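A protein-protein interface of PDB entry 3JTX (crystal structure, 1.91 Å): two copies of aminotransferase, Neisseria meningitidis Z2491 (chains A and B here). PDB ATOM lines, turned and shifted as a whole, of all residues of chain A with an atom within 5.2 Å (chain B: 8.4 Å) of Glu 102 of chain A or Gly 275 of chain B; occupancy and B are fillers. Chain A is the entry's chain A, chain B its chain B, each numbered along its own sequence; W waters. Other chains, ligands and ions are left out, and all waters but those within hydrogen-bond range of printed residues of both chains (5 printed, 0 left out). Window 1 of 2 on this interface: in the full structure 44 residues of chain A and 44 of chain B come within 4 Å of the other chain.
Printed residues of chain B that touch a printed residue of chain A: Glu 102, Tyr 270, Thr 272, Tyr 273, His 274 and Gly 275.
Hydrophobic or aromatic side chains of chain B within 4 Å of the printed part of chain A: Tyr 270, Tyr 273 and His 274.
Of the 15 printed residues of chain A, 4 touch a printed residue of chain B.
Among the printed residues, 10 pairs touch across the chains.
Among the printed residues, no Asp or Glu carboxylate lies within 4 Å of a Lys or Arg side-chain nitrogen of the other chain.
Water W2 lies within hydrogen-bond range of O of Leu 98 of chain A (2.7 Å), O of Gly 275 of chain B (2.8 Å), NH2 of Arg 253 of chain A (3.0 Å) and N of Glu 102 of chain A (3.1 Å).
Water W4 lies within hydrogen-bond range of O of His 274 of chain A (2.7 Å), O of Glu 102 of chain B (2.8 Å) and NE2 of His 274 of chain B (2.8 Å).
Water W1 lies within hydrogen-bond range of O of Ala 277 of chain B, O of Gly 275 of chain B and NE of Arg 253 of chain A.
Water W5 lies within hydrogen-bond range of O of His 274 of chain B, NE2 of His 274 of chain A and O of Glu 102 of chain A.
Water W3 bridges the backbone carbonyl oxygen of Leu 98 of chain A (2.9 Å) and the backbone carbonyl oxygen of Gly 275 of chain B (3.3 Å).
The backbone carbonyl oxygen (O) of Glu 102 of chain B lies within hydrogen-bond range of the side-chain hydroxyl (OG) of Ser 106 of chain B (2.8 Å).
A ring nitrogen (ND1) of His 274 of chain A is in hydrogen-bond range of the side-chain hydroxyl (OG) of Ser 276 of chain A (2.9 Å).
OE2 of Glu 102 of chain B is in hydrogen-bond range of N of Leu 98 of chain B (2.8 Å).
The backbone NH (N) of Leu 98 of chain A sits at hydrogen-bond distance from the side-chain carboxylate (OE2) of Glu 102 of chain A (2.8 Å).
The side-chain hydroxyl (OG1) of Thr 272 of chain B sits at hydrogen-bond distance from the backbone carbonyl oxygen (O) of Leu 268 of chain B (3.0 Å).
The backbone carbonyl oxygen (O) of Glu 102 of chain A lies within hydrogen-bond range of the side-chain hydroxyl (OG) of Ser 106 of chain A (2.7 Å).
Among the printed residues, pairs that only touch across the chains: His 274 of chain A with Glu 102 of chain B, Glu 102 of chain A with His 274 of chain B, Phe 105 of chain A with Tyr 273 of chain B, Phe 105 of chain A with Tyr 270 of chain B, His 274 of chain A with His 274 of chain B, Arg 101 of chain A with Gly 275 of chain B, Phe 105 of chain A with His 274 of chain B, Glu 102 of chain A with Gly 275 of chain B and Arg 101 of chain A with Tyr 273 of chain B.
Glu 102 of chain A touches just these residues of chain B: His 274 and Gly 275.
Gly 275 of chain B touches just these residues of chain A: Arg 101 (3.6 Å) and Glu 102 (3.7 Å).
No residue of chain B comes within 4 Å of Ala 103 of chain A.
Of the printed residues of chain A, Tyr 270 of chain B touches Phe 105.
Of the printed residues of chain A, Tyr 273 of chain B touches Arg 101 and Phe 105.
Of the printed residues of chain B, Arg 101 of chain A touches Thr 272, Tyr 273 and Gly 275.
The nearest residue of chain A that does not touch Gly 275 of chain B is Leu 98 of chain A (4.5 Å).
The nearest printed residue of chain B that does not touch His 274 of chain A is Ser 106 of chain B (5.8 Å).
Glu 102 of chain A touches His 274 of chain B, and with the chains exchanged His 274 of chain A touches Glu 102 of chain B.
His 274 of chain A touches its own counterpart, His 274 of chain B.
Positions printed for both chains: 98, 102, 106, 271, 274 and 276.
NH1 of Arg 101 of chain A is in hydrogen-bond range of O of Thr 272 of chain B (2.9 Å).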
ATOM      1  N   VAL A  97     -17.026  35.223 -24.016  1.00  0.00           N
ATOM      2  CA  VAL A  97     -17.475  33.879 -23.657  1.00  0.00           C
ATOM      3  C   VAL A  97     -17.709  33.779 -22.148  1.00  0.00           C
ATOM      4  O   VAL A  97     -17.136  34.537 -21.374  1.00  0.00           O
ATOM      5  CB  VAL A  97     -16.458  32.813 -24.104  1.00  0.00           C
ATOM      6  CG1 VAL A  97     -16.302  32.813 -25.643  1.00  0.00           C
ATOM      7  CG2 VAL A  97     -15.096  33.022 -23.416  1.00  0.00           C
ATOM      8  N   LEU A  98     -18.546  32.836 -21.733  1.00  0.00           N
ATOM      9  CA  LEU A  98     -18.975  32.732 -20.332  1.00  0.00           C
ATOM     10  C   LEU A  98     -18.017  31.816 -19.560  1.00  0.00           C
ATOM     11  O   LEU A  98     -18.413  30.751 -19.049  1.00  0.00           O
ATOM     12  CB  LEU A  98     -20.429  32.238 -20.242  1.00  0.00           C
ATOM     13  CG  LEU A  98     -21.415  32.982 -21.176  1.00  0.00           C
ATOM     14  CD1 LEU A  98     -22.860  32.512 -20.941  1.00  0.00           C
ATOM     15  CD2 LEU A  98     -21.302  34.517 -20.997  1.00  0.00           C
ATOM     16  N   GLY A  99     -16.758  32.241 -19.515  1.00  0.00           N
ATOM     17  CA  GLY A  99     -15.657  31.392 -19.068  1.00  0.00           C
ATOM     18  C   GLY A  99     -15.094  30.600 -20.227  1.00  0.00           C
ATOM     19  O   GLY A  99     -15.819  30.277 -21.184  1.00  0.00           O
ATOM     20  N   SER A 100     -13.797  30.285 -20.173  1.00  0.00           N
ATOM     21  CA  SER A 100     -13.180  29.543 -21.271  1.00  0.00           C
ATOM     22  C   SER A 100     -13.715  28.110 -21.368  1.00  0.00           C
ATOM     23  O   SER A 100     -13.703  27.528 -22.455  1.00  0.00           O
ATOM     24  CB  SER A 100     -11.643  29.547 -21.168  1.00  0.00           C
ATOM     25  OG  SER A 100     -11.185  28.817 -20.042  1.00  0.00           O
ATOM     26  N   ARG A 101     -14.182  27.523 -20.260  1.00  0.00           N
ATOM     27  CA  ARG A 101     -14.670  26.129 -20.315  1.00  0.00           C
ATOM     28  C   ARG A 101     -15.759  25.926 -21.379  1.00  0.00           C
ATOM     29  O   ARG A 101     -15.598  25.103 -22.288  1.00  0.00           O
ATOM     30  CB  ARG A 101     -15.200  25.670 -18.952  1.00  0.00           C
ATOM     31  CG  ARG A 101     -15.779  24.244 -18.977  1.00  0.00           C
ATOM     32  CD  ARG A 101     -16.056  23.706 -17.573  1.00  0.00           C
ATOM     33  NE  ARG A 101     -14.787  23.558 -16.876  1.00  0.00           N
ATOM     34  CZ  ARG A 101     -14.314  22.431 -16.358  1.00  0.00           C
ATOM     35  NH1 ARG A 101     -15.024  21.299 -16.362  1.00  0.00           N
ATOM     36  NH2 ARG A 101     -13.111  22.451 -15.801  1.00  0.00           N
ATOM     37  N   GLU A 102     -16.864  26.676 -21.282  1.00  0.00           N
ATOM     38  CA  GLU A 102     -17.959  26.522 -22.241  1.00  0.00           C
ATOM     39  C   GLU A 102     -17.488  26.805 -23.666  1.00  0.00           C
ATOM     40  O   GLU A 102     -17.950  26.172 -24.615  1.00  0.00           O
ATOM     41  CB  GLU A 102     -19.188  27.380 -21.865  1.00  0.00           C
ATOM     42  CG  GLU A 102     -18.988  28.888 -21.946  1.00  0.00           C
ATOM     43  CD  GLU A 102     -19.326  29.523 -23.313  1.00  0.00           C
ATOM     44  OE1 GLU A 102     -19.591  28.803 -24.296  1.00  0.00           O
ATOM     45  OE2 GLU A 102     -19.324  30.770 -23.396  1.00  0.00           O
ATOM     46  N   ALA A 103     -16.572  27.757 -23.797  1.00  0.00           N
ATOM     47  CA  ALA A 103     -16.045  28.203 -25.078  1.00  0.00           C
ATOM     48  C   ALA A 103     -15.223  27.107 -25.748  1.00  0.00           C
ATOM     49  O   ALA A 103     -15.432  26.799 -26.906  1.00  0.00           O
ATOM     50  CB  ALA A 103     -15.181  29.464 -24.873  1.00  0.00           C
ATOM     51  N   LEU A 104     -14.311  26.501 -24.993  1.00  0.00           N
ATOM     52  CA  LEU A 104     -13.470  25.435 -25.521  1.00  0.00           C
ATOM     53  C   LEU A 104     -14.338  24.229 -25.891  1.00  0.00           C
ATOM     54  O   LEU A 104     -14.167  23.631 -26.961  1.00  0.00           O
ATOM     55  CB  LEU A 104     -12.428  25.010 -24.476  1.00  0.00           C
ATOM     56  CG  LEU A 104     -11.283  25.970 -24.177  1.00  0.00           C
ATOM     57  CD1 LEU A 104     -10.691  25.706 -22.777  1.00  0.00           C
ATOM     58  CD2 LEU A 104     -10.191  25.897 -25.265  1.00  0.00           C
ATOM     59  N   PHE A 105     -15.269  23.876 -25.003  1.00  0.00           N
ATOM     60  CA  PHE A 105     -16.149  22.732 -25.239  1.00  0.00           C
ATOM     61  C   PHE A 105     -16.998  22.916 -26.491  1.00  0.00           C
ATOM     62  O   PHE A 105     -17.021  22.056 -27.384  1.00  0.00           O
ATOM     63  CB  PHE A 105     -17.060  22.470 -24.029  1.00  0.00           C
ATOM     64  CG  PHE A 105     -17.956  21.266 -24.217  1.00  0.00           C
ATOM     65  CD1 PHE A 105     -17.516  20.004 -23.866  1.00  0.00           C
ATOM     66  CD2 PHE A 105     -19.217  21.398 -24.783  1.00  0.00           C
ATOM     67  CE1 PHE A 105     -18.326  18.866 -24.066  1.00  0.00           C
ATOM     68  CE2 PHE A 105     -20.048  20.268 -24.978  1.00  0.00           C
ATOM     69  CZ  PHE A 105     -19.582  19.003 -24.630  1.00  0.00           C
ATOM     70  N   SER A 106     -17.709  24.042 -26.567  1.00  0.00           N
ATOM     71  CA  SER A 106     -18.586  24.284 -27.704  1.00  0.00           C
ATOM     72  C   SER A 106     -17.811  24.434 -29.017  1.00  0.00           C
ATOM     73  O   SER A 106     -18.251  23.921 -30.052  1.00  0.00           O
ATOM     74  CB  SER A 106     -19.491  25.497 -27.465  1.00  0.00           C
ATOM     75  OG  SER A 106     -18.748  26.660 -27.192  1.00  0.00           O
ATOM     76  N   PHE A 107     -16.655  25.093 -28.995  1.00  0.00           N
ATOM     77  CA  PHE A 107     -15.891  25.219 -30.221  1.00  0.00           C
ATOM     78  C   PHE A 107     -15.503  23.845 -30.779  1.00  0.00           C
ATOM     79  O   PHE A 107     -15.667  23.571 -31.965  1.00  0.00           O
ATOM     80  CB  PHE A 107     -14.658  26.125 -30.080  1.00  0.00           C
ATOM     81  CG  PHE A 107     -14.015  26.403 -31.401  1.00  0.00           C
ATOM     82  CD1 PHE A 107     -14.654  27.221 -32.329  1.00  0.00           C
ATOM     83  CD2 PHE A 107     -12.830  25.783 -31.765  1.00  0.00           C
ATOM     84  CE1 PHE A 107     -14.124  27.432 -33.591  1.00  0.00           C
ATOM     85  CE2 PHE A 107     -12.281  25.998 -33.036  1.00  0.00           C
ATOM     86  CZ  PHE A 107     -12.919  26.812 -33.939  1.00  0.00           C
ATOM     87  N   ARG A 253     -17.577  33.929 -14.514  1.00  0.00           N
ATOM     88  CA  ARG A 253     -17.773  33.155 -15.743  1.00  0.00           C
ATOM     89  C   ARG A 253     -17.653  34.107 -16.924  1.00  0.00           C
ATOM     90  O   ARG A 253     -18.641  34.347 -17.626  1.00  0.00           O
ATOM     91  CB  ARG A 253     -19.126  32.399 -15.774  1.00  0.00           C
ATOM     92  CG  ARG A 253     -19.468  31.598 -14.532  1.00  0.00           C
ATOM     93  CD  ARG A 253     -18.325  30.676 -14.056  1.00  0.00           C
ATOM     94  NE  ARG A 253     -17.840  29.800 -15.120  1.00  0.00           N
ATOM     95  CZ  ARG A 253     -16.566  29.604 -15.469  1.00  0.00           C
ATOM     96  NH1 ARG A 253     -15.549  30.186 -14.839  1.00  0.00           N
ATOM     97  NH2 ARG A 253     -16.295  28.774 -16.470  1.00  0.00           N
ATOM     98  N   ARG A 271     -23.503  29.809 -31.373  1.00  0.00           N
ATOM     99  CA  ARG A 271     -23.654  30.269 -30.004  1.00  0.00           C
ATOM    100  C   ARG A 271     -24.995  30.961 -29.773  1.00  0.00           C
ATOM    101  O   ARG A 271     -25.479  30.997 -28.641  1.00  0.00           O
ATOM    102  CB  ARG A 271     -22.490  31.173 -29.580  1.00  0.00           C
ATOM    103  CG  ARG A 271     -21.171  30.423 -29.449  1.00  0.00           C
ATOM    104  CD  ARG A 271     -19.988  31.354 -29.270  1.00  0.00           C
ATOM    105  NE  ARG A 271     -20.050  31.992 -27.968  1.00  0.00           N
ATOM    106  CZ  ARG A 271     -19.772  31.403 -26.818  1.00  0.00           C
ATOM    107  NH1 ARG A 271     -19.373  30.140 -26.774  1.00  0.00           N
ATOM    108  NH2 ARG A 271     -19.881  32.093 -25.704  1.00  0.00           N
ATOM    109  N   HIS A 274     -26.835  27.899 -28.879  1.00  0.00           N
ATOM    110  CA  HIS A 274     -26.199  27.253 -27.718  1.00  0.00           C
ATOM    111  C   HIS A 274     -26.464  28.036 -26.418  1.00  0.00           C
ATOM    112  O   HIS A 274     -26.381  27.473 -25.313  1.00  0.00           O
ATOM    113  CB  HIS A 274     -24.712  27.084 -28.078  1.00  0.00           C
ATOM    114  CG  HIS A 274     -23.781  26.810 -26.945  1.00  0.00           C
ATOM    115  ND1 HIS A 274     -22.960  27.787 -26.407  1.00  0.00           N
ATOM    116  CD2 HIS A 274     -23.425  25.646 -26.350  1.00  0.00           C
ATOM    117  CE1 HIS A 274     -22.184  27.240 -25.485  1.00  0.00           C
ATOM    118  NE2 HIS A 274     -22.457  25.946 -25.421  1.00  0.00           N
ATOM    119  N   SER A 276     -25.246  31.230 -25.084  1.00  0.00           N
ATOM    120  CA  SER A 276     -24.071  31.672 -24.333  1.00  0.00           C
ATOM    121  C   SER A 276     -23.809  33.189 -24.419  1.00  0.00           C
ATOM    122  O   SER A 276     -22.672  33.636 -24.438  1.00  0.00           O
ATOM    123  CB  SER A 276     -22.849  30.847 -24.750  1.00  0.00           C
ATOM    124  OG  SER A 276     -22.758  30.651 -26.171  1.00  0.00           O
ATOM    125  N   PRO B  63     -18.150  27.789  -8.932  1.00  0.00           N
ATOM    126  CA  PRO B  63     -19.368  27.092  -8.530  1.00  0.00           C
ATOM    127  C   PRO B  63     -19.403  25.664  -9.060  1.00  0.00           C
ATOM    128  O   PRO B  63     -18.877  25.395 -10.143  1.00  0.00           O
ATOM    129  CB  PRO B  63     -20.452  27.896  -9.220  1.00  0.00           C
ATOM    130  CG  PRO B  63     -19.805  28.403 -10.451  1.00  0.00           C
ATOM    131  CD  PRO B  63     -18.365  28.626 -10.120  1.00  0.00           C
ATOM    132  N   THR B  65     -21.383  22.544 -10.792  1.00  0.00           N
ATOM    133  CA  THR B  65     -22.408  22.487 -11.837  1.00  0.00           C
ATOM    134  C   THR B  65     -23.832  22.209 -11.298  1.00  0.00           C
ATOM    135  O   THR B  65     -24.811  22.769 -11.786  1.00  0.00           O
ATOM    136  CB  THR B  65     -22.005  21.444 -12.890  1.00  0.00           C
ATOM    137  OG1 THR B  65     -20.674  21.727 -13.324  1.00  0.00           O
ATOM    138  CG2 THR B  65     -22.943  21.473 -14.089  1.00  0.00           C
ATOM    139  N   LEU B  98     -28.535  28.034 -16.880  1.00  0.00           N
ATOM    140  CA  LEU B  98     -28.118  29.430 -17.096  1.00  0.00           C
ATOM    141  C   LEU B  98     -29.053  30.058 -18.118  1.00  0.00           C
ATOM    142  O   LEU B  98     -28.619  30.526 -19.170  1.00  0.00           O
ATOM    143  CB  LEU B  98     -26.651  29.502 -17.534  1.00  0.00           C
ATOM    144  CG  LEU B  98     -25.663  28.719 -16.647  1.00  0.00           C
ATOM    145  CD1 LEU B  98     -24.176  28.906 -17.060  1.00  0.00           C
ATOM    146  CD2 LEU B  98     -25.851  29.052 -15.169  1.00  0.00           C
ATOM    147  N   GLU B 102     -29.870  27.668 -23.051  1.00  0.00           N
ATOM    148  CA  GLU B 102     -28.708  26.777 -23.060  1.00  0.00           C
ATOM    149  C   GLU B 102     -29.119  25.369 -22.622  1.00  0.00           C
ATOM    150  O   GLU B 102     -28.575  24.382 -23.130  1.00  0.00           O
ATOM    151  CB  GLU B 102     -27.543  27.323 -22.192  1.00  0.00           C
ATOM    152  CG  GLU B 102     -27.818  27.376 -20.693  1.00  0.00           C
ATOM    153  CD  GLU B 102     -27.501  26.113 -19.912  1.00  0.00           C
ATOM    154  OE1 GLU B 102     -27.169  25.068 -20.519  1.00  0.00           O
ATOM    155  OE2 GLU B 102     -27.576  26.173 -18.664  1.00  0.00           O
ATOM    156  N   SER B 106     -28.579  22.156 -25.003  1.00  0.00           N
ATOM    157  CA  SER B 106     -27.639  21.118 -24.557  1.00  0.00           C
ATOM    158  C   SER B 106     -28.352  19.768 -24.308  1.00  0.00           C
ATOM    159  O   SER B 106     -27.831  18.692 -24.667  1.00  0.00           O
ATOM    160  CB  SER B 106     -26.858  21.567 -23.321  1.00  0.00           C
ATOM    161  OG  SER B 106     -27.695  21.876 -22.205  1.00  0.00           O
ATOM    162  N   LEU B 268     -26.297  16.230 -15.775  1.00  0.00           N
ATOM    163  CA  LEU B 268     -25.307  16.894 -14.904  1.00  0.00           C
ATOM    164  C   LEU B 268     -23.872  16.533 -15.306  1.00  0.00           C
ATOM    165  O   LEU B 268     -22.995  17.410 -15.355  1.00  0.00           O
ATOM    166  CB  LEU B 268     -25.528  16.528 -13.418  1.00  0.00           C
ATOM    167  CG  LEU B 268     -24.491  17.051 -12.404  1.00  0.00           C
ATOM    168  CD1 LEU B 268     -24.361  18.550 -12.517  1.00  0.00           C
ATOM    169  CD2 LEU B 268     -24.886  16.635 -10.959  1.00  0.00           C
ATOM    170  N   LEU B 269     -23.616  15.262 -15.593  1.00  0.00           N
ATOM    171  CA  LEU B 269     -22.273  14.851 -15.949  1.00  0.00           C
ATOM    172  C   LEU B 269     -21.850  15.574 -17.215  1.00  0.00           C
ATOM    173  O   LEU B 269     -20.716  16.055 -17.310  1.00  0.00           O
ATOM    174  CB  LEU B 269     -22.174  13.338 -16.178  1.00  0.00           C
ATOM    175  CG  LEU B 269     -22.432  12.450 -14.952  1.00  0.00           C
ATOM    176  CD1 LEU B 269     -22.400  10.971 -15.369  1.00  0.00           C
ATOM    177  CD2 LEU B 269     -21.463  12.765 -13.777  1.00  0.00           C
ATOM    178  N   TYR B 270     -22.759  15.649 -18.183  1.00  0.00           N
ATOM    179  CA  TYR B 270     -22.470  16.355 -19.436  1.00  0.00           C
ATOM    180  C   TYR B 270     -22.193  17.840 -19.190  1.00  0.00           C
ATOM    181  O   TYR B 270     -21.221  18.398 -19.693  1.00  0.00           O
ATOM    182  CB  TYR B 270     -23.648  16.217 -20.389  1.00  0.00           C
ATOM    183  CG  TYR B 270     -23.480  16.895 -21.719  1.00  0.00           C
ATOM    184  CD1 TYR B 270     -22.839  16.243 -22.772  1.00  0.00           C
ATOM    185  CD2 TYR B 270     -23.994  18.157 -21.955  1.00  0.00           C
ATOM    186  CE1 TYR B 270     -22.700  16.835 -24.005  1.00  0.00           C
ATOM    187  CE2 TYR B 270     -23.849  18.764 -23.213  1.00  0.00           C
ATOM    188  CZ  TYR B 270     -23.209  18.087 -24.219  1.00  0.00           C
ATOM    189  OH  TYR B 270     -23.068  18.647 -25.468  1.00  0.00           O
ATOM    190  N   ARG B 271     -23.041  18.457 -18.383  1.00  0.00           N
ATOM    191  CA  ARG B 271     -22.973  19.895 -18.111  1.00  0.00           C
ATOM    192  C   ARG B 271     -21.677  20.311 -17.413  1.00  0.00           C
ATOM    193  O   ARG B 271     -21.252  21.459 -17.534  1.00  0.00           O
ATOM    194  CB  ARG B 271     -24.199  20.333 -17.312  1.00  0.00           C
ATOM    195  CG  ARG B 271     -25.488  20.230 -18.119  1.00  0.00           C
ATOM    196  CD  ARG B 271     -26.751  20.493 -17.283  1.00  0.00           C
ATOM    197  NE  ARG B 271     -26.749  21.860 -16.789  1.00  0.00           N
ATOM    198  CZ  ARG B 271     -27.002  22.938 -17.533  1.00  0.00           C
ATOM    199  NH1 ARG B 271     -27.340  22.831 -18.824  1.00  0.00           N
ATOM    200  NH2 ARG B 271     -26.933  24.124 -16.977  1.00  0.00           N
ATOM    201  N   THR B 272     -21.050  19.394 -16.686  1.00  0.00           N
ATOM    202  CA  THR B 272     -19.770  19.677 -16.052  1.00  0.00           C
ATOM    203  C   THR B 272     -18.703  19.990 -17.102  1.00  0.00           C
ATOM    204  O   THR B 272     -17.849  20.835 -16.876  1.00  0.00           O
ATOM    205  CB  THR B 272     -19.308  18.506 -15.166  1.00  0.00           C
ATOM    206  OG1 THR B 272     -20.319  18.232 -14.190  1.00  0.00           O
ATOM    207  CG2 THR B 272     -17.997  18.834 -14.475  1.00  0.00           C
ATOM    208  N   TYR B 273     -18.786  19.321 -18.257  1.00  0.00           N
ATOM    209  CA  TYR B 273     -17.899  19.570 -19.389  1.00  0.00           C
ATOM    210  C   TYR B 273     -18.375  20.732 -20.285  1.00  0.00           C
ATOM    211  O   TYR B 273     -17.574  21.521 -20.789  1.00  0.00           O
ATOM    212  CB  TYR B 273     -17.737  18.289 -20.225  1.00  0.00           C
ATOM    213  CG  TYR B 273     -16.848  17.280 -19.572  1.00  0.00           C
ATOM    214  CD1 TYR B 273     -15.474  17.376 -19.699  1.00  0.00           C
ATOM    215  CD2 TYR B 273     -17.362  16.244 -18.804  1.00  0.00           C
ATOM    216  CE1 TYR B 273     -14.618  16.479 -19.107  1.00  0.00           C
ATOM    217  CE2 TYR B 273     -16.493  15.318 -18.193  1.00  0.00           C
ATOM    218  CZ  TYR B 273     -15.132  15.451 -18.351  1.00  0.00           C
ATOM    219  OH  TYR B 273     -14.236  14.557 -17.780  1.00  0.00           O
ATOM    220  N   HIS B 274     -19.680  20.822 -20.466  1.00  0.00           N
ATOM    221  CA  HIS B 274     -20.313  21.825 -21.301  1.00  0.00           C
ATOM    222  C   HIS B 274     -20.151  23.234 -20.689  1.00  0.00           C
ATOM    223  O   HIS B 274     -20.261  24.215 -21.396  1.00  0.00           O
ATOM    224  CB  HIS B 274     -21.769  21.380 -21.512  1.00  0.00           C
ATOM    225  CG  HIS B 274     -22.729  22.440 -21.951  1.00  0.00           C
ATOM    226  ND1 HIS B 274     -23.584  23.070 -21.074  1.00  0.00           N
ATOM    227  CD2 HIS B 274     -23.057  22.896 -23.188  1.00  0.00           C
ATOM    228  CE1 HIS B 274     -24.359  23.910 -21.738  1.00  0.00           C
ATOM    229  NE2 HIS B 274     -24.077  23.809 -23.026  1.00  0.00           N
ATOM    230  N   GLY B 275     -19.848  23.309 -19.387  1.00  0.00           N
ATOM    231  CA  GLY B 275     -19.370  24.536 -18.765  1.00  0.00           C
ATOM    232  C   GLY B 275     -20.497  25.460 -18.330  1.00  0.00           C
ATOM    233  O   GLY B 275     -20.373  26.701 -18.416  1.00  0.00           O
ATOM    234  N   SER B 276     -21.572  24.869 -17.803  1.00  0.00           N
ATOM    235  CA  SER B 276     -22.778  25.644 -17.486  1.00  0.00           C
ATOM    236  C   SER B 276     -23.116  25.689 -15.980  1.00  0.00           C
ATOM    237  O   SER B 276     -24.272  25.611 -15.607  1.00  0.00           O
ATOM    238  CB  SER B 276     -23.964  25.106 -18.310  1.00  0.00           C
ATOM    239  OG  SER B 276     -24.020  23.675 -18.284  1.00  0.00           O
ATOM    240  N   ALA B 277     -22.095  25.858 -15.147  1.00  0.00           N
ATOM    241  CA  ALA B 277     -22.256  26.080 -13.716  1.00  0.00           C
ATOM    242  C   ALA B 277     -22.597  27.545 -13.455  1.00  0.00           C
ATOM    243  O   ALA B 277     -22.057  28.430 -14.118  1.00  0.00           O
ATOM    244  CB  ALA B 277     -20.979  25.707 -12.993  1.00  0.00           C
ATOM    245  N   MET B 278     -23.451  27.800 -12.458  1.00  0.00           N
ATOM    246  CA  MET B 278     -23.926  29.152 -12.175  1.00  0.00           C
ATOM    247  C   MET B 278     -23.094  29.908 -11.129  1.00  0.00           C
ATOM    248  O   MET B 278     -22.866  29.419 -10.007  1.00  0.00           O
ATOM    249  CB  MET B 278     -25.383  29.093 -11.727  1.00  0.00           C
ATOM    250  CG  MET B 278     -26.079  30.439 -11.576  1.00  0.00           C
ATOM    251  SD  MET B 278     -27.928  30.229 -10.993  1.00  0.00           S
ATOM    252  CE  MET B 278     -28.720  29.518 -12.633  1.00  0.00           C
HETATM  253  O   HOH W   1     -20.112  28.214 -16.017  1.00  0.00           O
HETATM  254  O   HOH W   2     -17.974  28.100 -18.813  1.00  0.00           O
HETATM  255  O   HOH W   3     -20.934  29.961 -17.927  1.00  0.00           O
HETATM  256  O   HOH W   4     -26.209  24.864 -24.574  1.00  0.00           O
HETATM  257  O   HOH W   5     -20.367  24.575 -24.115  1.00  0.00           O
